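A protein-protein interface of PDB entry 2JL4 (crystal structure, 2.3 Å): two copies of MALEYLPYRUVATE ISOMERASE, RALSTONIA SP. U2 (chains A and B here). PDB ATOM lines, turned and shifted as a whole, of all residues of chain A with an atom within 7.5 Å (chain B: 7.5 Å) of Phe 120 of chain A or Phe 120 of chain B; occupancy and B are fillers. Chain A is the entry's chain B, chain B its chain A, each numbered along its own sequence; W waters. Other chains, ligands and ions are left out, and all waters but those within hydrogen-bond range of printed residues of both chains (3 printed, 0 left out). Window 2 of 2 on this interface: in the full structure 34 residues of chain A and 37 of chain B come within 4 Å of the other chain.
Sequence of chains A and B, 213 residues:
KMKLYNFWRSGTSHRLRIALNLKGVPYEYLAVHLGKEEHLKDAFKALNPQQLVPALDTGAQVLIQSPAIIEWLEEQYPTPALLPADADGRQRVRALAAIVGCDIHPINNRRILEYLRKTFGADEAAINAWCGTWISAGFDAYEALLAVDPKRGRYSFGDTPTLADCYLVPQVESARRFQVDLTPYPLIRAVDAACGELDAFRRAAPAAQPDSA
OG1 of Thr 119 of chain B sits close to O of Tyr 115 of chain B (3.5 Å). O of Leu 116 of chain B lies within hydrogen-bond range of N of Gly 121 of chain B (3.0 Å). The backbone carbonyl oxygen of Leu 116 of chain B sits at hydrogen-bond distance from the backbone NH of Ala 122 of chain B, 2.9 Å away. The backbone carbonyl oxygen (O) of Leu 116 of chain A is in hydrogen-bond range of the backbone NH (N) of Gly 121 of chain A, at 3.1 Å. The backbone carbonyl oxygen (O) of Leu 116 of chain A is in hydrogen-bond range of the backbone NH (N) of Ala 122 of chain A (2.9 Å).
OH of Tyr 115 of chain A touches C of Ala 129 of chain B (3.6 Å). CE3 of Trp 130 of chain B touches CD2 of Tyr 115 of chain A (3.3 Å). Leu 116 of chain A touches Leu 116 of chain B (CD2 to CD2, 3.8 Å). Phe 120 of chain A touches Phe 120 of chain B. Ala 122 of chain A touches Phe 120 of chain B (CB to CE1, 3.7 Å). Ala 129 of chain A touches Tyr 115 of chain B (C to OH, 3.7 Å). Trp 130 of chain A touches Ile 112 of chain B (CH2 to CG2, 3.6 Å). CE3 of Trp 130 of chain A touches CD2 of Tyr 115 of chain B (3.4 Å). CZ3 of Trp 130 of chain A touches CD2 of Leu 116 of chain B, 3.8 Å away. Trp 130 of chain A touches Phe 120 of chain B (CE3 to CE2, 3.9 Å).
Printed residues of chain B within 4 Å of Ile 112 of chain A: Trp 130 (3.6 Å). Printed residues of chain B within 4 Å of Leu 116 of chain A: Leu 116 and Phe 120. Printed residues of chain B within 4 Å of Phe 120 of chain A: Phe 120, Ala 122 and Trp 130. Of the printed residues of chain B, Ala 122 of chain A touches Phe 120 (3.7 Å). Printed residues of chain A within 4 Å of Phe 120 of chain B: Leu 116 (3.9 Å), Phe 120 (3.997 Å), Ala 122 (3.7 Å) and Trp 130 (3.9 Å). The nearest printed residue of chain B that does not touch Phe 120 of chain A is Leu 116 of chain B (4.1 Å). The nearest printed residue of chain A that does not touch Phe 120 of chain B is Ala 126 of chain A (4.2 Å).
Of the 16 printed residues of chain B, 7 touch a printed residue of chain A. Hydrophobic or aromatic side chains of chain B that line the printed part of chain A: Ile 112, Tyr 115, Leu 116, Phe 120, Ala 122 and Trp 130. Of the 16 printed residues of chain A, 7 touch a printed residue of chain B. Hydrophobic or aromatic side chains of chain A that line the printed part of chain B: Ile 112, Tyr 115, Leu 116, Phe 120, Ala 122 and Trp 130. Among the printed residues, no Asp or Glu carboxylate lies within 4 Å of a Lys or Arg side-chain nitrogen of the other chain.
Tyr 115 of chain A touches Trp 130 of chain B, and with the chains exchanged Trp 130 of chain A touches Tyr 115 of chain B. Leu 116 of chain A touches Phe 120 of chain B, but with the chains exchanged Phe 120 of chain A does not touch Leu 116 of chain B (4.1 Å). Phe 120 of chain B touches its own counterpart, Phe 120 of chain A. Trp 130 of chain A touches Leu 116 of chain B, but with the chains exchanged Leu 116 of chain A does not touch Trp 130 of chain B (4.002 Å). 16 positions are printed for both chains.
Water W1 lies within hydrogen-bond range of the side-chain hydroxyl (OH) of Tyr 115 of chain B (2.5 Å) and the backbone carbonyl oxygen (O) of Ala 126 of chain A (2.8 Å). Water W3 lies within hydrogen-bond range of the side-chain hydroxyl of Tyr 115 of chain A (2.6 Å) and the backbone carbonyl oxygen of Ala 126 of chain B (2.8 Å). Water W2 bridges O of Phe 120 of chain B (2.8 Å) and O of Phe 120 of chain A (2.9 Å).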
ATOM      1  N   ILE A 112      16.446 -16.779 -17.337  1.00  0.00           N
ATOM      2  CA  ILE A 112      17.668 -17.561 -17.232  1.00  0.00           C
ATOM      3  C   ILE A 112      17.885 -17.935 -15.772  1.00  0.00           C
ATOM      4  O   ILE A 112      18.124 -19.102 -15.448  1.00  0.00           O
ATOM      5  CB  ILE A 112      18.915 -16.766 -17.743  1.00  0.00           C
ATOM      6  CG1 ILE A 112      18.681 -16.163 -19.146  1.00  0.00           C
ATOM      7  CG2 ILE A 112      20.177 -17.621 -17.680  1.00  0.00           C
ATOM      8  CD1 ILE A 112      18.313 -17.157 -20.260  1.00  0.00           C
ATOM      9  N   LEU A 113      17.795 -16.939 -14.896  1.00  0.00           N
ATOM     10  CA  LEU A 113      18.061 -17.152 -13.476  1.00  0.00           C
ATOM     11  C   LEU A 113      17.031 -18.104 -12.897  1.00  0.00           C
ATOM     12  O   LEU A 113      17.346 -18.904 -12.026  1.00  0.00           O
ATOM     13  CB  LEU A 113      18.096 -15.828 -12.708  1.00  0.00           C
ATOM     14  CG  LEU A 113      18.998 -14.716 -13.284  1.00  0.00           C
ATOM     15  CD1 LEU A 113      19.023 -13.524 -12.339  1.00  0.00           C
ATOM     16  CD2 LEU A 113      20.431 -15.194 -13.570  1.00  0.00           C
ATOM     17  N   GLU A 114      15.810 -18.032 -13.418  1.00  0.00           N
ATOM     18  CA  GLU A 114      14.744 -18.957 -13.048  1.00  0.00           C
ATOM     19  C   GLU A 114      15.058 -20.385 -13.467  1.00  0.00           C
ATOM     20  O   GLU A 114      14.797 -21.328 -12.711  1.00  0.00           O
ATOM     21  CB  GLU A 114      13.414 -18.505 -13.656  1.00  0.00           C
ATOM     22  CG  GLU A 114      12.766 -17.391 -12.866  1.00  0.00           C
ATOM     23  CD  GLU A 114      12.234 -17.873 -11.521  1.00  0.00           C
ATOM     24  OE1 GLU A 114      11.326 -18.723 -11.526  1.00  0.00           O
ATOM     25  OE2 GLU A 114      12.715 -17.407 -10.465  1.00  0.00           O
ATOM     26  N   TYR A 115      15.613 -20.533 -14.675  1.00  0.00           N
ATOM     27  CA  TYR A 115      16.076 -21.831 -15.175  1.00  0.00           C
ATOM     28  C   TYR A 115      17.152 -22.414 -14.250  1.00  0.00           C
ATOM     29  O   TYR A 115      17.076 -23.581 -13.866  1.00  0.00           O
ATOM     30  CB  TYR A 115      16.597 -21.715 -16.614  1.00  0.00           C
ATOM     31  CG  TYR A 115      16.634 -23.029 -17.368  1.00  0.00           C
ATOM     32  CD1 TYR A 115      15.641 -23.357 -18.290  1.00  0.00           C
ATOM     33  CD2 TYR A 115      17.659 -23.959 -17.149  1.00  0.00           C
ATOM     34  CE1 TYR A 115      15.680 -24.574 -18.991  1.00  0.00           C
ATOM     35  CE2 TYR A 115      17.701 -25.176 -17.842  1.00  0.00           C
ATOM     36  CZ  TYR A 115      16.723 -25.470 -18.752  1.00  0.00           C
ATOM     37  OH  TYR A 115      16.785 -26.664 -19.425  1.00  0.00           O
ATOM     38  N   LEU A 116      18.133 -21.587 -13.883  1.00  0.00           N
ATOM     39  CA  LEU A 116      19.206 -21.990 -12.970  1.00  0.00           C
ATOM     40  C   LEU A 116      18.673 -22.425 -11.603  1.00  0.00           C
ATOM     41  O   LEU A 116      19.200 -23.343 -10.997  1.00  0.00           O
ATOM     42  CB  LEU A 116      20.250 -20.866 -12.789  1.00  0.00           C
ATOM     43  CG  LEU A 116      21.036 -20.342 -13.995  1.00  0.00           C
ATOM     44  CD1 LEU A 116      21.770 -19.078 -13.600  1.00  0.00           C
ATOM     45  CD2 LEU A 116      22.009 -21.366 -14.594  1.00  0.00           C
ATOM     46  N   ARG A 117      17.630 -21.753 -11.129  1.00  0.00           N
ATOM     47  CA  ARG A 117      17.000 -22.094  -9.866  1.00  0.00           C
ATOM     48  C   ARG A 117      16.240 -23.409  -9.996  1.00  0.00           C
ATOM     49  O   ARG A 117      16.462 -24.336  -9.230  1.00  0.00           O
ATOM     50  CB  ARG A 117      16.060 -20.971  -9.425  1.00  0.00           C
ATOM     51  CG  ARG A 117      16.768 -19.748  -8.881  1.00  0.00           C
ATOM     52  CD  ARG A 117      15.781 -18.681  -8.364  1.00  0.00           C
ATOM     53  NE  ARG A 117      16.422 -17.370  -8.235  1.00  0.00           N
ATOM     54  CZ  ARG A 117      16.177 -16.315  -9.013  1.00  0.00           C
ATOM     55  NH1 ARG A 117      15.264 -16.369  -9.982  1.00  0.00           N
ATOM     56  NH2 ARG A 117      16.843 -15.183  -8.805  1.00  0.00           N
ATOM     57  N   LYS A 118      15.362 -23.501 -10.992  1.00  0.00           N
ATOM     58  CA  LYS A 118      14.403 -24.604 -11.057  1.00  0.00           C
ATOM     59  C   LYS A 118      14.964 -25.889 -11.669  1.00  0.00           C
ATOM     60  O   LYS A 118      14.576 -26.991 -11.272  1.00  0.00           O
ATOM     61  CB  LYS A 118      13.115 -24.156 -11.749  1.00  0.00           C
ATOM     62  CG  LYS A 118      12.412 -23.029 -11.004  1.00  0.00           C
ATOM     63  CD  LYS A 118      10.940 -22.961 -11.344  1.00  0.00           C
ATOM     64  CE  LYS A 118      10.304 -21.711 -10.769  1.00  0.00           C
ATOM     65  NZ  LYS A 118       8.896 -21.542 -11.255  1.00  0.00           N
ATOM     66  N   THR A 119      15.897 -25.752 -12.604  1.00  0.00           N
ATOM     67  CA  THR A 119      16.531 -26.913 -13.222  1.00  0.00           C
ATOM     68  C   THR A 119      17.884 -27.267 -12.581  1.00  0.00           C
ATOM     69  O   THR A 119      18.220 -28.442 -12.453  1.00  0.00           O
ATOM     70  CB  THR A 119      16.662 -26.713 -14.746  1.00  0.00           C
ATOM     71  OG1 THR A 119      15.354 -26.499 -15.298  1.00  0.00           O
ATOM     72  CG2 THR A 119      17.300 -27.931 -15.429  1.00  0.00           C
ATOM     73  N   PHE A 120      18.654 -26.264 -12.174  1.00  0.00           N
ATOM     74  CA  PHE A 120      19.996 -26.529 -11.656  1.00  0.00           C
ATOM     75  C   PHE A 120      20.136 -26.323 -10.139  1.00  0.00           C
ATOM     76  O   PHE A 120      21.240 -26.434  -9.586  1.00  0.00           O
ATOM     77  CB  PHE A 120      21.059 -25.760 -12.453  1.00  0.00           C
ATOM     78  CG  PHE A 120      21.182 -26.213 -13.889  1.00  0.00           C
ATOM     79  CD1 PHE A 120      21.616 -27.499 -14.195  1.00  0.00           C
ATOM     80  CD2 PHE A 120      20.867 -25.354 -14.930  1.00  0.00           C
ATOM     81  CE1 PHE A 120      21.722 -27.924 -15.515  1.00  0.00           C
ATOM     82  CE2 PHE A 120      20.974 -25.768 -16.256  1.00  0.00           C
ATOM     83  CZ  PHE A 120      21.397 -27.057 -16.547  1.00  0.00           C
ATOM     84  N   GLY A 121      19.008 -26.024  -9.491  1.00  0.00           N
ATOM     85  CA  GLY A 121      18.912 -25.949  -8.037  1.00  0.00           C
ATOM     86  C   GLY A 121      19.655 -24.796  -7.406  1.00  0.00           C
ATOM     87  O   GLY A 121      19.889 -24.803  -6.189  1.00  0.00           O
ATOM     88  N   ALA A 122      20.027 -23.806  -8.225  1.00  0.00           N
ATOM     89  CA  ALA A 122      20.854 -22.683  -7.782  1.00  0.00           C
ATOM     90  C   ALA A 122      20.210 -21.867  -6.661  1.00  0.00           C
ATOM     91  O   ALA A 122      19.032 -21.508  -6.736  1.00  0.00           O
ATOM     92  CB  ALA A 122      21.204 -21.783  -8.965  1.00  0.00           C
ATOM     93  N   ASP A 123      20.977 -21.585  -5.612  1.00  0.00           N
ATOM     94  CA  ASP A 123      20.494 -20.664  -4.583  1.00  0.00           C
ATOM     95  C   ASP A 123      20.936 -19.254  -4.947  1.00  0.00           C
ATOM     96  O   ASP A 123      21.578 -19.057  -5.986  1.00  0.00           O
ATOM     97  CB  ASP A 123      20.889 -21.098  -3.154  1.00  0.00           C
ATOM     98  CG  ASP A 123      22.403 -21.071  -2.884  1.00  0.00           C
ATOM     99  OD1 ASP A 123      23.234 -20.624  -3.716  1.00  0.00           O
ATOM    100  OD2 ASP A 123      22.766 -21.511  -1.777  1.00  0.00           O
ATOM    101  N   ALA A 126      24.740 -18.493  -5.711  1.00  0.00           N
ATOM    102  CA  ALA A 126      25.145 -19.047  -6.990  1.00  0.00           C
ATOM    103  C   ALA A 126      24.587 -18.200  -8.132  1.00  0.00           C
ATOM    104  O   ALA A 126      25.244 -18.038  -9.157  1.00  0.00           O
ATOM    105  CB  ALA A 126      24.685 -20.482  -7.113  1.00  0.00           C
ATOM    106  N   ILE A 127      23.378 -17.659  -7.945  1.00  0.00           N
ATOM    107  CA  ILE A 127      22.794 -16.695  -8.890  1.00  0.00           C
ATOM    108  C   ILE A 127      23.668 -15.433  -9.013  1.00  0.00           C
ATOM    109  O   ILE A 127      23.961 -14.983 -10.137  1.00  0.00           O
ATOM    110  CB  ILE A 127      21.345 -16.296  -8.500  1.00  0.00           C
ATOM    111  CG1 ILE A 127      20.381 -17.491  -8.643  1.00  0.00           C
ATOM    112  CG2 ILE A 127      20.874 -15.039  -9.281  1.00  0.00           C
ATOM    113  CD1 ILE A 127      20.132 -17.975 -10.057  1.00  0.00           C
ATOM    114  N   ALA A 129      26.817 -15.134  -8.238  1.00  0.00           N
ATOM    115  CA  ALA A 129      28.145 -15.500  -8.745  1.00  0.00           C
ATOM    116  C   ALA A 129      28.142 -15.590 -10.271  1.00  0.00           C
ATOM    117  O   ALA A 129      29.127 -15.207 -10.923  1.00  0.00           O
ATOM    118  CB  ALA A 129      28.631 -16.806  -8.120  1.00  0.00           C
ATOM    119  N   TRP A 130      27.024 -16.095 -10.804  1.00  0.00           N
ATOM    120  CA  TRP A 130      26.723 -16.182 -12.233  1.00  0.00           C
ATOM    121  C   TRP A 130      26.625 -14.813 -12.889  1.00  0.00           C
ATOM    122  O   TRP A 130      27.251 -14.563 -13.922  1.00  0.00           O
ATOM    123  CB  TRP A 130      25.400 -16.937 -12.414  1.00  0.00           C
ATOM    124  CG  TRP A 130      24.776 -16.916 -13.796  1.00  0.00           C
ATOM    125  CD1 TRP A 130      23.958 -15.948 -14.318  1.00  0.00           C
ATOM    126  CD2 TRP A 130      24.864 -17.944 -14.797  1.00  0.00           C
ATOM    127  NE1 TRP A 130      23.550 -16.298 -15.585  1.00  0.00           N
ATOM    128  CE2 TRP A 130      24.089 -17.519 -15.904  1.00  0.00           C
ATOM    129  CE3 TRP A 130      25.527 -19.181 -14.867  1.00  0.00           C
ATOM    130  CZ2 TRP A 130      23.962 -18.286 -17.073  1.00  0.00           C
ATOM    131  CZ3 TRP A 130      25.401 -19.944 -16.032  1.00  0.00           C
ATOM    132  CH2 TRP A 130      24.620 -19.493 -17.115  1.00  0.00           C
ATOM    133  N   ILE B 112      29.248 -20.220 -21.530  1.00  0.00           N
ATOM    134  CA  ILE B 112      28.046 -20.438 -20.716  1.00  0.00           C
ATOM    135  C   ILE B 112      27.848 -21.933 -20.443  1.00  0.00           C
ATOM    136  O   ILE B 112      27.602 -22.338 -19.310  1.00  0.00           O
ATOM    137  CB  ILE B 112      26.752 -19.885 -21.411  1.00  0.00           C
ATOM    138  CG1 ILE B 112      26.908 -18.424 -21.900  1.00  0.00           C
ATOM    139  CG2 ILE B 112      25.517 -20.065 -20.513  1.00  0.00           C
ATOM    140  CD1 ILE B 112      27.347 -17.391 -20.851  1.00  0.00           C
ATOM    141  N   LEU B 113      27.951 -22.746 -21.491  1.00  0.00           N
ATOM    142  CA  LEU B 113      27.758 -24.193 -21.361  1.00  0.00           C
ATOM    143  C   LEU B 113      28.840 -24.787 -20.462  1.00  0.00           C
ATOM    144  O   LEU B 113      28.575 -25.685 -19.656  1.00  0.00           O
ATOM    145  CB  LEU B 113      27.736 -24.868 -22.742  1.00  0.00           C
ATOM    146  CG  LEU B 113      26.745 -24.281 -23.760  1.00  0.00           C
ATOM    147  CD1 LEU B 113      26.747 -25.103 -25.039  1.00  0.00           C
ATOM    148  CD2 LEU B 113      25.314 -24.174 -23.198  1.00  0.00           C
ATOM    149  N   GLU B 114      30.049 -24.243 -20.590  1.00  0.00           N
ATOM    150  CA  GLU B 114      31.168 -24.610 -19.736  1.00  0.00           C
ATOM    151  C   GLU B 114      30.892 -24.285 -18.278  1.00  0.00           C
ATOM    152  O   GLU B 114      31.208 -25.087 -17.388  1.00  0.00           O
ATOM    153  CB  GLU B 114      32.445 -23.911 -20.204  1.00  0.00           C
ATOM    154  CG  GLU B 114      33.085 -24.592 -21.400  1.00  0.00           C
ATOM    155  CD  GLU B 114      33.589 -25.974 -21.053  1.00  0.00           C
ATOM    156  OE1 GLU B 114      34.598 -26.057 -20.323  1.00  0.00           O
ATOM    157  OE2 GLU B 114      32.972 -26.968 -21.501  1.00  0.00           O
ATOM    158  N   TYR B 115      30.304 -23.111 -18.040  1.00  0.00           N
ATOM    159  CA  TYR B 115      29.883 -22.727 -16.691  1.00  0.00           C
ATOM    160  C   TYR B 115      28.847 -23.714 -16.140  1.00  0.00           C
ATOM    161  O   TYR B 115      28.981 -24.181 -15.015  1.00  0.00           O
ATOM    162  CB  TYR B 115      29.377 -21.281 -16.672  1.00  0.00           C
ATOM    163  CG  TYR B 115      29.323 -20.646 -15.302  1.00  0.00           C
ATOM    164  CD1 TYR B 115      30.271 -19.703 -14.907  1.00  0.00           C
ATOM    165  CD2 TYR B 115      28.319 -20.983 -14.398  1.00  0.00           C
ATOM    166  CE1 TYR B 115      30.211 -19.115 -13.644  1.00  0.00           C
ATOM    167  CE2 TYR B 115      28.249 -20.400 -13.141  1.00  0.00           C
ATOM    168  CZ  TYR B 115      29.188 -19.473 -12.770  1.00  0.00           C
ATOM    169  OH  TYR B 115      29.084 -18.904 -11.530  1.00  0.00           O
ATOM    170  N   LEU B 116      27.842 -24.060 -16.944  1.00  0.00           N
ATOM    171  CA  LEU B 116      26.838 -25.078 -16.554  1.00  0.00           C
ATOM    172  C   LEU B 116      27.468 -26.437 -16.211  1.00  0.00           C
ATOM    173  O   LEU B 116      27.084 -27.076 -15.221  1.00  0.00           O
ATOM    174  CB  LEU B 116      25.764 -25.264 -17.633  1.00  0.00           C
ATOM    175  CG  LEU B 116      24.998 -24.015 -18.096  1.00  0.00           C
ATOM    176  CD1 LEU B 116      24.116 -24.339 -19.294  1.00  0.00           C
ATOM    177  CD2 LEU B 116      24.165 -23.361 -16.990  1.00  0.00           C
ATOM    178  N   ARG B 117      28.430 -26.869 -17.025  1.00  0.00           N
ATOM    179  CA  ARG B 117      29.148 -28.114 -16.756  1.00  0.00           C
ATOM    180  C   ARG B 117      29.896 -28.007 -15.429  1.00  0.00           C
ATOM    181  O   ARG B 117      29.711 -28.826 -14.539  1.00  0.00           O
ATOM    182  CB  ARG B 117      30.118 -28.461 -17.900  1.00  0.00           C
ATOM    183  CG  ARG B 117      29.414 -28.884 -19.186  1.00  0.00           C
ATOM    184  CD  ARG B 117      30.372 -29.249 -20.337  1.00  0.00           C
ATOM    185  NE  ARG B 117      29.654 -29.373 -21.613  1.00  0.00           N
ATOM    186  CZ  ARG B 117      29.758 -28.531 -22.648  1.00  0.00           C
ATOM    187  NH1 ARG B 117      30.571 -27.476 -22.605  1.00  0.00           N
ATOM    188  NH2 ARG B 117      29.050 -28.755 -23.750  1.00  0.00           N
ATOM    189  N   LYS B 118      30.698 -26.959 -15.291  1.00  0.00           N
ATOM    190  CA  LYS B 118      31.721 -26.911 -14.262  1.00  0.00           C
ATOM    191  C   LYS B 118      31.229 -26.425 -12.886  1.00  0.00           C
ATOM    192  O   LYS B 118      31.750 -26.835 -11.848  1.00  0.00           O
ATOM    193  CB  LYS B 118      32.895 -26.078 -14.769  1.00  0.00           C
ATOM    194  CG  LYS B 118      34.227 -26.776 -14.608  1.00  0.00           C
ATOM    195  CD  LYS B 118      35.209 -26.358 -15.674  1.00  0.00           C
ATOM    196  CE  LYS B 118      34.936 -27.080 -16.970  1.00  0.00           C
ATOM    197  NZ  LYS B 118      36.116 -27.003 -17.864  1.00  0.00           N
ATOM    198  N   THR B 119      30.216 -25.563 -12.893  1.00  0.00           N
ATOM    199  CA  THR B 119      29.630 -25.033 -11.665  1.00  0.00           C
ATOM    200  C   THR B 119      28.333 -25.751 -11.286  1.00  0.00           C
ATOM    201  O   THR B 119      28.056 -25.964 -10.106  1.00  0.00           O
ATOM    202  CB  THR B 119      29.365 -23.533 -11.816  1.00  0.00           C
ATOM    203  OG1 THR B 119      30.584 -22.902 -12.206  1.00  0.00           O
ATOM    204  CG2 THR B 119      28.832 -22.907 -10.505  1.00  0.00           C
ATOM    205  N   PHE B 120      27.541 -26.118 -12.281  1.00  0.00           N
ATOM    206  CA  PHE B 120      26.273 -26.773 -12.009  1.00  0.00           C
ATOM    207  C   PHE B 120      26.248 -28.253 -12.374  1.00  0.00           C
ATOM    208  O   PHE B 120      25.211 -28.902 -12.248  1.00  0.00           O
ATOM    209  CB  PHE B 120      25.120 -26.013 -12.671  1.00  0.00           C
ATOM    210  CG  PHE B 120      24.959 -24.607 -12.162  1.00  0.00           C
ATOM    211  CD1 PHE B 120      24.461 -24.369 -10.882  1.00  0.00           C
ATOM    212  CD2 PHE B 120      25.302 -23.524 -12.960  1.00  0.00           C
ATOM    213  CE1 PHE B 120      24.307 -23.079 -10.413  1.00  0.00           C
ATOM    214  CE2 PHE B 120      25.145 -22.227 -12.499  1.00  0.00           C
ATOM    215  CZ  PHE B 120      24.648 -22.006 -11.223  1.00  0.00           C
ATOM    216  N   GLY B 121      27.388 -28.781 -12.821  1.00  0.00           N
ATOM    217  CA  GLY B 121      27.541 -30.220 -13.073  1.00  0.00           C
ATOM    218  C   GLY B 121      26.653 -30.766 -14.174  1.00  0.00           C
ATOM    219  O   GLY B 121      26.378 -31.978 -14.224  1.00  0.00           O
ATOM    220  N   ALA B 122      26.192 -29.872 -15.048  1.00  0.00           N
ATOM    221  CA  ALA B 122      25.354 -30.247 -16.181  1.00  0.00           C
ATOM    222  C   ALA B 122      26.054 -31.277 -17.057  1.00  0.00           C
ATOM    223  O   ALA B 122      27.247 -31.154 -17.347  1.00  0.00           O
ATOM    224  CB  ALA B 122      24.976 -29.015 -17.003  1.00  0.00           C
ATOM    225  N   ASP B 123      25.315 -32.307 -17.445  1.00  0.00           N
ATOM    226  CA  ASP B 123      25.805 -33.263 -18.431  1.00  0.00           C
ATOM    227  C   ASP B 123      25.232 -32.881 -19.793  1.00  0.00           C
ATOM    228  O   ASP B 123      24.445 -31.939 -19.878  1.00  0.00           O
ATOM    229  CB  ASP B 123      25.481 -34.709 -18.021  1.00  0.00           C
ATOM    230  CG  ASP B 123      23.997 -35.054 -18.126  1.00  0.00           C
ATOM    231  OD1 ASP B 123      23.147 -34.163 -18.372  1.00  0.00           O
ATOM    232  OD2 ASP B 123      23.684 -36.252 -17.953  1.00  0.00           O
ATOM    233  N   ALA B 126      21.412 -32.280 -20.397  1.00  0.00           N
ATOM    234  CA  ALA B 126      20.991 -31.056 -19.739  1.00  0.00           C
ATOM    235  C   ALA B 126      21.449 -29.834 -20.533  1.00  0.00           C
ATOM    236  O   ALA B 126      20.698 -28.859 -20.654  1.00  0.00           O
ATOM    237  CB  ALA B 126      21.522 -31.003 -18.313  1.00  0.00           C
ATOM    238  N   ILE B 127      22.675 -29.894 -21.067  1.00  0.00           N
ATOM    239  CA  ILE B 127      23.185 -28.873 -21.995  1.00  0.00           C
ATOM    240  C   ILE B 127      22.254 -28.719 -23.208  1.00  0.00           C
ATOM    241  O   ILE B 127      21.868 -27.592 -23.562  1.00  0.00           O
ATOM    242  CB  ILE B 127      24.639 -29.174 -22.474  1.00  0.00           C
ATOM    243  CG1 ILE B 127      25.647 -29.009 -21.328  1.00  0.00           C
ATOM    244  CG2 ILE B 127      25.029 -28.306 -23.696  1.00  0.00           C
ATOM    245  CD1 ILE B 127      25.762 -27.578 -20.766  1.00  0.00           C
ATOM    246  N   ALA B 129      19.126 -29.619 -23.453  1.00  0.00           N
ATOM    247  CA  ALA B 129      17.811 -29.156 -22.998  1.00  0.00           C
ATOM    248  C   ALA B 129      17.794 -27.639 -22.782  1.00  0.00           C
ATOM    249  O   ALA B 129      16.807 -26.976 -23.106  1.00  0.00           O
ATOM    250  CB  ALA B 129      17.370 -29.904 -21.729  1.00  0.00           C
ATOM    251  N   TRP B 130      18.897 -27.121 -22.230  1.00  0.00           N
ATOM    252  CA  TRP B 130      19.154 -25.688 -22.092  1.00  0.00           C
ATOM    253  C   TRP B 130      19.121 -24.972 -23.448  1.00  0.00           C
ATOM    254  O   TRP B 130      18.339 -24.030 -23.646  1.00  0.00           O
ATOM    255  CB  TRP B 130      20.518 -25.500 -21.424  1.00  0.00           C
ATOM    256  CG  TRP B 130      21.066 -24.094 -21.350  1.00  0.00           C
ATOM    257  CD1 TRP B 130      21.836 -23.459 -22.291  1.00  0.00           C
ATOM    258  CD2 TRP B 130      20.938 -23.173 -20.255  1.00  0.00           C
ATOM    259  NE1 TRP B 130      22.174 -22.197 -21.859  1.00  0.00           N
ATOM    260  CE2 TRP B 130      21.644 -21.997 -20.611  1.00  0.00           C
ATOM    261  CE3 TRP B 130      20.300 -23.227 -19.005  1.00  0.00           C
ATOM    262  CZ2 TRP B 130      21.725 -20.885 -19.764  1.00  0.00           C
ATOM    263  CZ3 TRP B 130      20.375 -22.115 -18.170  1.00  0.00           C
ATOM    264  CH2 TRP B 130      21.081 -20.963 -18.554  1.00  0.00           C
HETATM  265  O   HOH W   1      27.287 -19.711  -9.959  1.00  0.00           O
HETATM  266  O   HOH W   2      23.380 -28.208 -10.255  1.00  0.00           O
HETATM  267  O   HOH W   3      18.844 -28.113 -18.695  1.00  0.00           O
